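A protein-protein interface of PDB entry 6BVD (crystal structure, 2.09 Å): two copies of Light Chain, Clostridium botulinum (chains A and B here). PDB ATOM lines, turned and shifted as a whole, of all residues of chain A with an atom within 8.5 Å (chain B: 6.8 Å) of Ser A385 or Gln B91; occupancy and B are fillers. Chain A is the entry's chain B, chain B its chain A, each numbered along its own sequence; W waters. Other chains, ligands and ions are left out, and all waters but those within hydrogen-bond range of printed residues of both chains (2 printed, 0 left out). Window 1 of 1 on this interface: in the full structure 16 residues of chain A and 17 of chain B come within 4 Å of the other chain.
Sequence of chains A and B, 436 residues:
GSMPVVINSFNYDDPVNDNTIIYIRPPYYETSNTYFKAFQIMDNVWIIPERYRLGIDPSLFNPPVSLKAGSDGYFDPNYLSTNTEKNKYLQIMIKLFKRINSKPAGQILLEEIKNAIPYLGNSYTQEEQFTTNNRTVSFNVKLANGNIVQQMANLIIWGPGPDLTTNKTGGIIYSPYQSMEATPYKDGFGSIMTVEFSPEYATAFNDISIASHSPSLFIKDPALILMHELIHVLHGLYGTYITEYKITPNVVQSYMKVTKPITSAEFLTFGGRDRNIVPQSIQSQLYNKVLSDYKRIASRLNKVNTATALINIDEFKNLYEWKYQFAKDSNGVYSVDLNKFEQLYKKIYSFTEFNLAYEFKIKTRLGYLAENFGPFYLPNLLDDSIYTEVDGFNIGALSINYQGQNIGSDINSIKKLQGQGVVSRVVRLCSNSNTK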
ATOM      1  N   LYS A  95     -19.516 -21.794 -11.015  1.00  0.00           N
ATOM      2  CA  LYS A  95     -19.601 -22.005  -9.556  1.00  0.00           C
ATOM      3  C   LYS A  95     -18.229 -22.341  -8.923  1.00  0.00           C
ATOM      4  O   LYS A  95     -17.916 -21.848  -7.843  1.00  0.00           O
ATOM      5  CB  LYS A  95     -20.615 -23.093  -9.260  1.00  0.00           C
ATOM      6  CG  LYS A  95     -21.035 -23.118  -7.765  1.00  0.00           C
ATOM      7  CD  LYS A  95     -22.291 -23.992  -7.533  1.00  0.00           C
ATOM      8  CE  LYS A  95     -22.735 -23.934  -6.066  1.00  0.00           C
ATOM      9  NZ  LYS A  95     -24.134 -24.391  -5.912  1.00  0.00           N
ATOM     10  N   ASN A 380     -25.357 -33.156  -8.274  1.00  0.00           N
ATOM     11  CA  ASN A 380     -25.993 -31.936  -7.821  1.00  0.00           C
ATOM     12  C   ASN A 380     -25.058 -30.831  -7.300  1.00  0.00           C
ATOM     13  O   ASN A 380     -25.368 -30.164  -6.331  1.00  0.00           O
ATOM     14  CB  ASN A 380     -27.026 -32.301  -6.736  1.00  0.00           C
ATOM     15  CG  ASN A 380     -28.053 -33.284  -7.236  1.00  0.00           C
ATOM     16  OD1 ASN A 380     -28.136 -34.431  -6.782  1.00  0.00           O
ATOM     17  ND2 ASN A 380     -28.849 -32.838  -8.183  1.00  0.00           N
ATOM     18  N   LEU A 381     -23.952 -30.584  -7.994  1.00  0.00           N
ATOM     19  CA  LEU A 381     -23.042 -29.526  -7.593  1.00  0.00           C
ATOM     20  C   LEU A 381     -23.732 -28.164  -7.673  1.00  0.00           C
ATOM     21  O   LEU A 381     -23.429 -27.275  -6.890  1.00  0.00           O
ATOM     22  CB  LEU A 381     -21.772 -29.549  -8.465  1.00  0.00           C
ATOM     23  CG  LEU A 381     -20.869 -30.792  -8.322  1.00  0.00           C
ATOM     24  CD1 LEU A 381     -19.753 -30.837  -9.380  1.00  0.00           C
ATOM     25  CD2 LEU A 381     -20.264 -30.825  -6.918  1.00  0.00           C
ATOM     26  N   LEU A 382     -24.695 -28.010  -8.592  1.00  0.00           N
ATOM     27  CA  LEU A 382     -25.391 -26.726  -8.749  1.00  0.00           C
ATOM     28  C   LEU A 382     -26.465 -26.475  -7.650  1.00  0.00           C
ATOM     29  O   LEU A 382     -26.958 -25.379  -7.513  1.00  0.00           O
ATOM     30  CB  LEU A 382     -26.050 -26.668 -10.131  1.00  0.00           C
ATOM     31  CG  LEU A 382     -25.070 -26.505 -11.304  1.00  0.00           C
ATOM     32  CD1 LEU A 382     -25.858 -26.737 -12.608  1.00  0.00           C
ATOM     33  CD2 LEU A 382     -24.477 -25.123 -11.274  1.00  0.00           C
ATOM     34  N   ASP A 383     -26.777 -27.491  -6.852  1.00  0.00           N
ATOM     35  CA  ASP A 383     -27.783 -27.381  -5.774  1.00  0.00           C
ATOM     36  C   ASP A 383     -27.162 -26.837  -4.479  1.00  0.00           C
ATOM     37  O   ASP A 383     -26.331 -27.508  -3.859  1.00  0.00           O
ATOM     38  CB  ASP A 383     -28.392 -28.751  -5.517  1.00  0.00           C
ATOM     39  CG  ASP A 383     -29.605 -28.708  -4.553  1.00  0.00           C
ATOM     40  OD1 ASP A 383     -29.725 -27.795  -3.706  1.00  0.00           O
ATOM     41  OD2 ASP A 383     -30.416 -29.639  -4.623  1.00  0.00           O
ATOM     42  N   ASP A 384     -27.550 -25.638  -4.075  1.00  0.00           N
ATOM     43  CA  ASP A 384     -26.904 -24.983  -2.929  1.00  0.00           C
ATOM     44  C   ASP A 384     -27.228 -25.678  -1.594  1.00  0.00           C
ATOM     45  O   ASP A 384     -26.615 -25.336  -0.590  1.00  0.00           O
ATOM     46  CB  ASP A 384     -27.305 -23.506  -2.834  1.00  0.00           C
ATOM     47  CG  ASP A 384     -26.491 -22.577  -3.788  1.00  0.00           C
ATOM     48  OD1 ASP A 384     -25.259 -22.685  -3.847  1.00  0.00           O
ATOM     49  OD2 ASP A 384     -27.080 -21.669  -4.407  1.00  0.00           O
ATOM     50  N   SER A 385     -28.173 -26.621  -1.583  1.00  0.00           N
ATOM     51  CA  SER A 385     -28.455 -27.388  -0.345  1.00  0.00           C
ATOM     52  C   SER A 385     -27.456 -28.545  -0.243  1.00  0.00           C
ATOM     53  O   SER A 385     -27.401 -29.250   0.774  1.00  0.00           O
ATOM     54  CB  SER A 385     -29.896 -27.916  -0.315  1.00  0.00           C
ATOM     55  OG  SER A 385     -30.098 -28.918  -1.309  1.00  0.00           O
ATOM     56  N   ILE A 386     -26.674 -28.745  -1.308  1.00  0.00           N
ATOM     57  CA  ILE A 386     -25.684 -29.815  -1.347  1.00  0.00           C
ATOM     58  C   ILE A 386     -24.246 -29.282  -1.359  1.00  0.00           C
ATOM     59  O   ILE A 386     -23.366 -29.788  -0.645  1.00  0.00           O
ATOM     60  CB  ILE A 386     -25.892 -30.736  -2.598  1.00  0.00           C
ATOM     61  CG1 ILE A 386     -27.278 -31.396  -2.606  1.00  0.00           C
ATOM     62  CG2 ILE A 386     -24.776 -31.756  -2.734  1.00  0.00           C
ATOM     63  CD1 ILE A 386     -27.528 -32.368  -1.490  1.00  0.00           C
ATOM     64  N   TYR A 387     -24.008 -28.273  -2.201  1.00  0.00           N
ATOM     65  CA  TYR A 387     -22.662 -27.755  -2.468  1.00  0.00           C
ATOM     66  C   TYR A 387     -22.748 -26.240  -2.715  1.00  0.00           C
ATOM     67  O   TYR A 387     -23.508 -25.803  -3.593  1.00  0.00           O
ATOM     68  CB  TYR A 387     -22.067 -28.493  -3.673  1.00  0.00           C
ATOM     69  CG  TYR A 387     -20.647 -28.128  -4.013  1.00  0.00           C
ATOM     70  CD1 TYR A 387     -19.579 -28.778  -3.413  1.00  0.00           C
ATOM     71  CD2 TYR A 387     -20.364 -27.133  -4.957  1.00  0.00           C
ATOM     72  CE1 TYR A 387     -18.253 -28.446  -3.747  1.00  0.00           C
ATOM     73  CE2 TYR A 387     -19.058 -26.795  -5.287  1.00  0.00           C
ATOM     74  CZ  TYR A 387     -17.997 -27.443  -4.676  1.00  0.00           C
ATOM     75  OH  TYR A 387     -16.676 -27.118  -5.014  1.00  0.00           O
ATOM     76  N   THR A 388     -22.030 -25.440  -1.930  1.00  0.00           N
ATOM     77  CA  THR A 388     -22.097 -23.985  -2.056  1.00  0.00           C
ATOM     78  C   THR A 388     -20.767 -23.421  -2.496  1.00  0.00           C
ATOM     79  O   THR A 388     -19.715 -24.086  -2.354  1.00  0.00           O
ATOM     80  CB  THR A 388     -22.491 -23.279  -0.750  1.00  0.00           C
ATOM     81  OG1 THR A 388     -21.576 -23.664   0.299  1.00  0.00           O
ATOM     82  CG2 THR A 388     -23.943 -23.631  -0.337  1.00  0.00           C
ATOM     83  N   ASP A 391     -18.810 -22.816   0.981  1.00  0.00           N
ATOM     84  CA  ASP A 391     -18.433 -23.926   1.885  1.00  0.00           C
ATOM     85  C   ASP A 391     -18.213 -25.280   1.226  1.00  0.00           C
ATOM     86  O   ASP A 391     -17.840 -26.246   1.904  1.00  0.00           O
ATOM     87  CB  ASP A 391     -19.502 -24.102   2.996  1.00  0.00           C
ATOM     88  CG  ASP A 391     -19.540 -22.949   3.980  1.00  0.00           C
ATOM     89  OD1 ASP A 391     -18.441 -22.434   4.270  1.00  0.00           O
ATOM     90  OD2 ASP A 391     -20.649 -22.596   4.517  1.00  0.00           O
ATOM     91  N   GLY A 392     -18.496 -25.392  -0.070  1.00  0.00           N
ATOM     92  CA  GLY A 392     -18.425 -26.684  -0.710  1.00  0.00           C
ATOM     93  C   GLY A 392     -19.470 -27.656  -0.125  1.00  0.00           C
ATOM     94  O   GLY A 392     -20.624 -27.289   0.073  1.00  0.00           O
ATOM     95  N   PHE A 393     -19.063 -28.900   0.158  1.00  0.00           N
ATOM     96  CA  PHE A 393     -19.989 -29.880   0.732  1.00  0.00           C
ATOM     97  C   PHE A 393     -20.189 -29.630   2.234  1.00  0.00           C
ATOM     98  O   PHE A 393     -21.213 -30.080   2.839  1.00  0.00           O
ATOM     99  CB  PHE A 393     -19.476 -31.315   0.519  1.00  0.00           C
ATOM    100  CG  PHE A 393     -19.397 -31.740  -0.933  1.00  0.00           C
ATOM    101  CD1 PHE A 393     -20.549 -31.998  -1.660  1.00  0.00           C
ATOM    102  CD2 PHE A 393     -18.168 -31.923  -1.545  1.00  0.00           C
ATOM    103  CE1 PHE A 393     -20.473 -32.412  -2.985  1.00  0.00           C
ATOM    104  CE2 PHE A 393     -18.080 -32.331  -2.878  1.00  0.00           C
ATOM    105  CZ  PHE A 393     -19.237 -32.579  -3.596  1.00  0.00           C
ATOM    106  N   ASN A 394     -19.235 -28.928   2.843  1.00  0.00           N
ATOM    107  CA  ASN A 394     -19.220 -28.852   4.330  1.00  0.00           C
ATOM    108  C   ASN A 394     -20.044 -27.660   4.865  1.00  0.00           C
ATOM    109  O   ASN A 394     -19.516 -26.711   5.480  1.00  0.00           O
ATOM    110  CB  ASN A 394     -17.764 -28.809   4.817  1.00  0.00           C
ATOM    111  CG  ASN A 394     -16.962 -30.057   4.401  1.00  0.00           C
ATOM    112  OD1 ASN A 394     -17.459 -31.181   4.441  1.00  0.00           O
ATOM    113  ND2 ASN A 394     -15.719 -29.841   3.945  1.00  0.00           N
ATOM    114  N   ILE A 395     -21.356 -27.712   4.599  1.00  0.00           N
ATOM    115  CA  ILE A 395     -22.298 -26.690   4.988  1.00  0.00           C
ATOM    116  C   ILE A 395     -22.721 -26.848   6.453  1.00  0.00           C
ATOM    117  O   ILE A 395     -23.113 -27.939   6.868  1.00  0.00           O
ATOM    118  CB  ILE A 395     -23.561 -26.757   4.129  1.00  0.00           C
ATOM    119  CG1 ILE A 395     -23.199 -26.699   2.633  1.00  0.00           C
ATOM    120  CG2 ILE A 395     -24.498 -25.668   4.525  1.00  0.00           C
ATOM    121  CD1 ILE A 395     -24.359 -27.133   1.783  1.00  0.00           C
ATOM    122  N   GLY A 396     -22.659 -25.760   7.214  1.00  0.00           N
ATOM    123  CA  GLY A 396     -23.103 -25.751   8.601  1.00  0.00           C
ATOM    124  C   GLY A 396     -22.288 -26.740   9.412  1.00  0.00           C
ATOM    125  O   GLY A 396     -21.083 -26.792   9.256  1.00  0.00           O
ATOM    126  N   LEU A 398     -21.778 -29.744   9.109  1.00  0.00           N
ATOM    127  CA  LEU A 398     -21.122 -30.779   8.337  1.00  0.00           C
ATOM    128  C   LEU A 398     -19.618 -30.478   8.219  1.00  0.00           C
ATOM    129  O   LEU A 398     -18.837 -31.335   7.825  1.00  0.00           O
ATOM    130  CB  LEU A 398     -21.764 -30.905   6.945  1.00  0.00           C
ATOM    131  CG  LEU A 398     -23.185 -31.490   6.886  1.00  0.00           C
ATOM    132  CD1 LEU A 398     -23.800 -31.226   5.519  1.00  0.00           C
ATOM    133  CD2 LEU A 398     -23.245 -32.996   7.226  1.00  0.00           C
ATOM    134  N   ARG A 425     -27.645 -37.897  -2.659  1.00  0.00           N
ATOM    135  CA  ARG A 425     -27.724 -36.736  -3.552  1.00  0.00           C
ATOM    136  C   ARG A 425     -26.355 -36.062  -3.677  1.00  0.00           C
ATOM    137  O   ARG A 425     -26.205 -35.040  -4.347  1.00  0.00           O
ATOM    138  CB  ARG A 425     -28.780 -35.735  -3.075  1.00  0.00           C
ATOM    139  CG  ARG A 425     -30.210 -36.145  -3.430  1.00  0.00           C
ATOM    140  CD  ARG A 425     -31.192 -34.979  -3.320  1.00  0.00           C
ATOM    141  NE  ARG A 425     -31.157 -34.142  -4.519  1.00  0.00           N
ATOM    142  CZ  ARG A 425     -30.900 -32.839  -4.517  1.00  0.00           C
ATOM    143  NH1 ARG A 425     -30.678 -32.204  -3.371  1.00  0.00           N
ATOM    144  NH2 ARG A 425     -30.875 -32.166  -5.660  1.00  0.00           N
ATOM    145  N   VAL A 426     -25.366 -36.645  -3.007  1.00  0.00           N
ATOM    146  CA  VAL A 426     -23.998 -36.150  -3.048  1.00  0.00           C
ATOM    147  C   VAL A 426     -23.176 -36.911  -4.102  1.00  0.00           C
ATOM    148  O   VAL A 426     -22.561 -36.300  -4.969  1.00  0.00           O
ATOM    149  CB  VAL A 426     -23.327 -36.260  -1.657  1.00  0.00           C
ATOM    150  CG1 VAL A 426     -21.950 -35.637  -1.680  1.00  0.00           C
ATOM    151  CG2 VAL A 426     -24.184 -35.579  -0.603  1.00  0.00           C
ATOM    152  N   SER B   9     -24.563 -20.189   7.836  1.00  0.00           N
ATOM    153  CA  SER B   9     -25.182 -21.398   7.261  1.00  0.00           C
ATOM    154  C   SER B   9     -25.389 -22.496   8.333  1.00  0.00           C
ATOM    155  O   SER B   9     -24.692 -22.529   9.349  1.00  0.00           O
ATOM    156  CB  SER B   9     -24.341 -21.957   6.101  1.00  0.00           C
ATOM    157  OG  SER B   9     -24.424 -21.101   4.966  1.00  0.00           O
ATOM    158  N   PHE B  10     -26.385 -23.347   8.106  1.00  0.00           N
ATOM    159  CA  PHE B  10     -26.796 -24.411   9.023  1.00  0.00           C
ATOM    160  C   PHE B  10     -27.705 -25.365   8.251  1.00  0.00           C
ATOM    161  O   PHE B  10     -28.334 -24.974   7.254  1.00  0.00           O
ATOM    162  CB  PHE B  10     -27.536 -23.850  10.271  1.00  0.00           C
ATOM    163  CG  PHE B  10     -28.134 -22.462  10.062  1.00  0.00           C
ATOM    164  CD1 PHE B  10     -29.158 -22.255   9.142  1.00  0.00           C
ATOM    165  CD2 PHE B  10     -27.640 -21.371  10.766  1.00  0.00           C
ATOM    166  CE1 PHE B  10     -29.696 -20.986   8.931  1.00  0.00           C
ATOM    167  CE2 PHE B  10     -28.170 -20.087  10.565  1.00  0.00           C
ATOM    168  CZ  PHE B  10     -29.209 -19.892   9.655  1.00  0.00           C
ATOM    169  N   ASN B  11     -27.764 -26.610   8.702  1.00  0.00           N
ATOM    170  CA  ASN B  11     -28.767 -27.559   8.232  1.00  0.00           C
ATOM    171  C   ASN B  11     -29.815 -27.726   9.336  1.00  0.00           C
ATOM    172  O   ASN B  11     -29.492 -27.514  10.505  1.00  0.00           O
ATOM    173  CB  ASN B  11     -28.105 -28.892   7.867  1.00  0.00           C
ATOM    174  CG  ASN B  11     -26.902 -28.698   6.964  1.00  0.00           C
ATOM    175  OD1 ASN B  11     -27.067 -28.454   5.782  1.00  0.00           O
ATOM    176  ND2 ASN B  11     -25.692 -28.811   7.519  1.00  0.00           N
ATOM    177  N   TYR B  12     -31.053 -28.086   8.991  1.00  0.00           N
ATOM    178  CA  TYR B  12     -32.092 -28.179  10.023  1.00  0.00           C
ATOM    179  C   TYR B  12     -31.689 -29.177  11.121  1.00  0.00           C
ATOM    180  O   TYR B  12     -32.025 -28.985  12.293  1.00  0.00           O
ATOM    181  CB  TYR B  12     -33.444 -28.596   9.435  1.00  0.00           C
ATOM    182  CG  TYR B  12     -34.535 -28.485  10.467  1.00  0.00           C
ATOM    183  CD1 TYR B  12     -35.075 -27.254  10.794  1.00  0.00           C
ATOM    184  CD2 TYR B  12     -34.970 -29.610  11.169  1.00  0.00           C
ATOM    185  CE1 TYR B  12     -36.061 -27.142  11.785  1.00  0.00           C
ATOM    186  CE2 TYR B  12     -35.945 -29.510  12.153  1.00  0.00           C
ATOM    187  CZ  TYR B  12     -36.487 -28.280  12.449  1.00  0.00           C
ATOM    188  OH  TYR B  12     -37.453 -28.180  13.429  1.00  0.00           O
ATOM    189  N   LYS B  86     -38.276 -28.407   5.831  1.00  0.00           N
ATOM    190  CA  LYS B  86     -37.829 -27.300   6.680  1.00  0.00           C
ATOM    191  C   LYS B  86     -36.370 -26.934   6.337  1.00  0.00           C
ATOM    192  O   LYS B  86     -35.982 -25.752   6.314  1.00  0.00           O
ATOM    193  CB  LYS B  86     -37.971 -27.669   8.174  1.00  0.00           C
ATOM    194  CG  LYS B  86     -39.415 -27.902   8.573  1.00  0.00           C
ATOM    195  CD  LYS B  86     -39.507 -28.137  10.116  1.00  0.00           C
ATOM    196  CE  LYS B  86     -40.927 -28.309  10.640  1.00  0.00           C
ATOM    197  NZ  LYS B  86     -41.552 -29.616  10.327  1.00  0.00           N
ATOM    198  N   ASN B  87     -35.564 -27.956   6.057  1.00  0.00           N
ATOM    199  CA  ASN B  87     -34.175 -27.718   5.708  1.00  0.00           C
ATOM    200  C   ASN B  87     -34.069 -27.009   4.353  1.00  0.00           C
ATOM    201  O   ASN B  87     -33.235 -26.136   4.163  1.00  0.00           O
ATOM    202  CB  ASN B  87     -33.390 -29.023   5.690  1.00  0.00           C
ATOM    203  CG  ASN B  87     -31.921 -28.800   5.368  1.00  0.00           C
ATOM    204  OD1 ASN B  87     -31.192 -28.195   6.153  1.00  0.00           O
ATOM    205  ND2 ASN B  87     -31.491 -29.248   4.201  1.00  0.00           N
ATOM    206  N   LYS B  88     -34.922 -27.398   3.417  1.00  0.00           N
ATOM    207  CA  LYS B  88     -34.921 -26.763   2.113  1.00  0.00           C
ATOM    208  C   LYS B  88     -35.243 -25.275   2.269  1.00  0.00           C
ATOM    209  O   LYS B  88     -34.548 -24.432   1.707  1.00  0.00           O
ATOM    210  CB  LYS B  88     -35.925 -27.447   1.176  1.00  0.00           C
ATOM    211  CG  LYS B  88     -35.738 -27.027  -0.276  1.00  0.00           C
ATOM    212  CD  LYS B  88     -36.930 -27.400  -1.138  1.00  0.00           C
ATOM    213  CE  LYS B  88     -36.703 -26.973  -2.591  1.00  0.00           C
ATOM    214  NZ  LYS B  88     -37.868 -27.329  -3.445  1.00  0.00           N
ATOM    215  N   TYR B  89     -36.270 -24.973   3.084  1.00  0.00           N
ATOM    216  CA  TYR B  89     -36.684 -23.609   3.406  1.00  0.00           C
ATOM    217  C   TYR B  89     -35.505 -22.812   4.005  1.00  0.00           C
ATOM    218  O   TYR B  89     -35.264 -21.655   3.640  1.00  0.00           O
ATOM    219  CB  TYR B  89     -37.907 -23.635   4.401  1.00  0.00           C
ATOM    220  CG  TYR B  89     -38.393 -22.281   4.817  1.00  0.00           C
ATOM    221  CD1 TYR B  89     -39.537 -21.711   4.239  1.00  0.00           C
ATOM    222  CD2 TYR B  89     -37.721 -21.564   5.813  1.00  0.00           C
ATOM    223  CE1 TYR B  89     -39.971 -20.450   4.611  1.00  0.00           C
ATOM    224  CE2 TYR B  89     -38.150 -20.315   6.201  1.00  0.00           C
ATOM    225  CZ  TYR B  89     -39.279 -19.768   5.613  1.00  0.00           C
ATOM    226  OH  TYR B  89     -39.685 -18.527   6.021  1.00  0.00           O
ATOM    227  N   LEU B  90     -34.797 -23.414   4.951  1.00  0.00           N
ATOM    228  CA  LEU B  90     -33.617 -22.787   5.530  1.00  0.00           C
ATOM    229  C   LEU B  90     -32.564 -22.458   4.439  1.00  0.00           C
ATOM    230  O   LEU B  90     -32.006 -21.382   4.432  1.00  0.00           O
ATOM    231  CB  LEU B  90     -32.967 -23.702   6.550  1.00  0.00           C
ATOM    232  CG  LEU B  90     -33.549 -23.724   7.953  1.00  0.00           C
ATOM    233  CD1 LEU B  90     -32.602 -24.535   8.880  1.00  0.00           C
ATOM    234  CD2 LEU B  90     -33.759 -22.309   8.463  1.00  0.00           C
ATOM    235  N   GLN B  91     -32.282 -23.402   3.553  1.00  0.00           N
ATOM    236  CA  GLN B  91     -31.242 -23.145   2.539  1.00  0.00           C
ATOM    237  C   GLN B  91     -31.631 -22.037   1.562  1.00  0.00           C
ATOM    238  O   GLN B  91     -30.769 -21.329   1.031  1.00  0.00           O
ATOM    239  CB  GLN B  91     -30.899 -24.420   1.761  1.00  0.00           C
ATOM    240  CG  GLN B  91     -30.546 -25.593   2.650  1.00  0.00           C
ATOM    241  CD  GLN B  91     -29.515 -25.265   3.715  1.00  0.00           C
ATOM    242  OE1 GLN B  91     -28.458 -24.717   3.427  1.00  0.00           O
ATOM    243  NE2 GLN B  91     -29.826 -25.624   4.977  1.00  0.00           N
ATOM    244  N   ILE B  92     -32.912 -21.937   1.245  1.00  0.00           N
ATOM    245  CA  ILE B  92     -33.359 -20.887   0.345  1.00  0.00           C
ATOM    246  C   ILE B  92     -33.206 -19.553   1.054  1.00  0.00           C
ATOM    247  O   ILE B  92     -32.744 -18.584   0.475  1.00  0.00           O
ATOM    248  CB  ILE B  92     -34.822 -21.150  -0.090  1.00  0.00           C
ATOM    249  CG1 ILE B  92     -34.857 -22.438  -0.906  1.00  0.00           C
ATOM    250  CG2 ILE B  92     -35.442 -19.919  -0.793  1.00  0.00           C
ATOM    251  CD1 ILE B  92     -36.257 -22.908  -1.265  1.00  0.00           C
ATOM    252  N   MET B  93     -33.578 -19.507   2.333  1.00  0.00           N
ATOM    253  CA  MET B  93     -33.466 -18.279   3.097  1.00  0.00           C
ATOM    254  C   MET B  93     -31.992 -17.841   3.181  1.00  0.00           C
ATOM    255  O   MET B  93     -31.677 -16.652   3.060  1.00  0.00           O
ATOM    256  CB  MET B  93     -34.071 -18.442   4.512  1.00  0.00           C
ATOM    257  CG  MET B  93     -35.565 -18.684   4.508  1.00  0.00           C
ATOM    258  SD  MET B  93     -36.476 -17.408   3.632  1.00  0.00           S
ATOM    259  CE  MET B  93     -36.047 -15.929   4.564  1.00  0.00           C
ATOM    260  N   ILE B  94     -31.093 -18.802   3.347  1.00  0.00           N
ATOM    261  CA  ILE B  94     -29.669 -18.510   3.339  1.00  0.00           C
ATOM    262  C   ILE B  94     -29.282 -17.900   1.976  1.00  0.00           C
ATOM    263  O   ILE B  94     -28.582 -16.900   1.871  1.00  0.00           O
ATOM    264  CB  ILE B  94     -28.866 -19.790   3.601  1.00  0.00           C
ATOM    265  CG1 ILE B  94     -28.976 -20.215   5.071  1.00  0.00           C
ATOM    266  CG2 ILE B  94     -27.410 -19.600   3.295  1.00  0.00           C
ATOM    267  CD1 ILE B  94     -28.427 -21.608   5.313  1.00  0.00           C
ATOM    268  N   LYS B  95     -29.806 -18.493   0.922  1.00  0.00           N
ATOM    269  CA  LYS B  95     -29.472 -17.984  -0.430  1.00  0.00           C
ATOM    270  C   LYS B  95     -30.004 -16.556  -0.633  1.00  0.00           C
ATOM    271  O   LYS B  95     -29.323 -15.679  -1.220  1.00  0.00           O
ATOM    272  CB  LYS B  95     -30.023 -18.937  -1.494  1.00  0.00           C
ATOM    273  CG  LYS B  95     -29.417 -18.686  -2.901  1.00  0.00           C
ATOM    274  CD  LYS B  95     -29.788 -19.788  -3.875  1.00  0.00           C
ATOM    275  CE  LYS B  95     -29.122 -19.504  -5.239  1.00  0.00           C
ATOM    276  NZ  LYS B  95     -29.118 -20.765  -5.982  1.00  0.00           N
ATOM    277  N   LEU B  96     -31.209 -16.296  -0.126  1.00  0.00           N
ATOM    278  CA  LEU B  96     -31.799 -14.969  -0.296  1.00  0.00           C
ATOM    279  C   LEU B  96     -31.089 -13.894   0.529  1.00  0.00           C
ATOM    280  O   LEU B  96     -30.870 -12.780   0.046  1.00  0.00           O
ATOM    281  CB  LEU B  96     -33.299 -14.990   0.038  1.00  0.00           C
ATOM    282  CG  LEU B  96     -34.155 -15.923  -0.815  1.00  0.00           C
ATOM    283  CD1 LEU B  96     -35.633 -15.816  -0.452  1.00  0.00           C
ATOM    284  CD2 LEU B  96     -34.011 -15.645  -2.346  1.00  0.00           C
ATOM    285  N   LYS B  98     -27.875 -14.078   1.323  1.00  0.00           N
ATOM    286  CA  LYS B  98     -26.612 -13.882   0.598  1.00  0.00           C
ATOM    287  C   LYS B  98     -26.821 -13.023  -0.655  1.00  0.00           C
ATOM    288  O   LYS B  98     -25.920 -12.286  -1.043  1.00  0.00           O
ATOM    289  CB  LYS B  98     -25.949 -15.216   0.216  1.00  0.00           C
ATOM    290  CG  LYS B  98     -25.285 -15.917   1.421  1.00  0.00           C
ATOM    291  CD  LYS B  98     -24.312 -17.041   1.067  1.00  0.00           C
ATOM    292  CE  LYS B  98     -25.004 -18.394   0.881  1.00  0.00           C
ATOM    293  NZ  LYS B  98     -24.098 -19.576   0.739  1.00  0.00           N
ATOM    294  N   LEU B 382     -32.775 -23.092  -5.525  1.00  0.00           N
ATOM    295  CA  LEU B 382     -31.470 -23.572  -5.044  1.00  0.00           C
ATOM    296  C   LEU B 382     -30.493 -23.952  -6.157  1.00  0.00           C
ATOM    297  O   LEU B 382     -29.312 -24.110  -5.891  1.00  0.00           O
ATOM    298  CB  LEU B 382     -31.667 -24.787  -4.129  1.00  0.00           C
ATOM    299  CG  LEU B 382     -32.246 -24.486  -2.749  1.00  0.00           C
ATOM    300  CD1 LEU B 382     -32.578 -25.799  -2.073  1.00  0.00           C
ATOM    301  CD2 LEU B 382     -31.202 -23.758  -1.971  1.00  0.00           C
HETATM  302  O   HOH W   1     -28.547 -28.681   3.338  1.00  0.00           O
HETATM  303  O   HOH W   2     -26.902 -23.489   1.715  1.00  0.00           O
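O of Leu B382 sits at hydrogen-bond distance from N of Asp A384.
The backbone carbonyl oxygen (O) of Leu A382 sits close to the backbone carbonyl oxygen (O) of Leu B382, at 3.1 Å.
ND2 of Asn B11 lies within hydrogen-bond range of O of Ile A395, 2.8 Å away.
The side-chain carboxylate (OD2) of Asp A384 sits close to the side-chain amino group (NZ) of Lys B95 (2.7 Å).
Leu B382 touches its own counterpart, Leu A382.
Positions printed for both chains: 95 and 382.
Water W2 lies within hydrogen-bond range of the side-chain amide oxygen (OE1) of Gln B91 (2.6 Å) and the backbone carbonyl oxygen (O) of Asp A384 (3.0 Å).
Water W1 lies within hydrogen-bond range of the side-chain amide oxygen of Asn B11 (2.9 Å), the backbone carbonyl oxygen of Ser A385 (2.9 Å) and the side-chain amide nitrogen of Asn B87 (3.1 Å).
Printed residues of chain B that touch a printed residue of chain A: Ser B9, Phe B10, Asn B11, Gln B91, Lys B95 and Leu B382.
Hydrophobic or aromatic side chains of chain B that line the printed part of chain A: Leu B382.
Among the printed residues, 10 pairs touch across the chains.
Among the printed residues, Asp or Glu carboxylates within 4 Å of a Lys or Arg side-chain nitrogen of the other chain: Asp A384 with Lys B95.
Of chain B, only Gln B91 and Leu B382 come within 4 Å of Ser A385.
Gln B91 touches one residue of chain A.
Of the printed residues of chain B, Asp A383 touches Leu B382 (3.6 Å).
Of the printed residues of chain B, Ile A395 touches Asn B11 (2.8 Å).
Met B93 touches none of the printed residues of chain A.
The nearest residue of chain B that does not touch Ser A385 is Asn B87 (5.0 Å).
The nearest residue of chain A that does not touch Gln B91 is Ile A395 (4.2 Å).
NE2 of Gln B91 sits at hydrogen-bond distance from O of Phe B10 (2.8 Å).
The side-chain carboxylate (OD2) of Asp A383 lies within salt-bridge range of the guanidinium group (NH2) of Arg A425.
OD1 of Asp A383 is in hydrogen-bond range of OG of Ser A385 (2.7 Å).
NE2 of Gln B91 lies within hydrogen-bond range of OD1 of Asn B87 (3.1 Å).
NZ of Lys B95 sits at hydrogen-bond distance from O of Leu B382, 3.4 Å away.
NZ of Lys A95 sits close to OD1 of Asp A384 (2.9 Å).
Leu B382 touches Asp A383 (CB to OD1, 3.6 Å).
Ser A385 touches Gln B91 (CB to CG, 3.8 Å).
Leu B382 touches Ser A385.
Gly A396 touches Ser B9 (CA to O, 3.7 Å).
Gly A396 touches Phe B10 (CA to CA, 3.95 Å).
CD1 of Leu A398 touches ND2 of Asn B11, 3.7 Å away.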
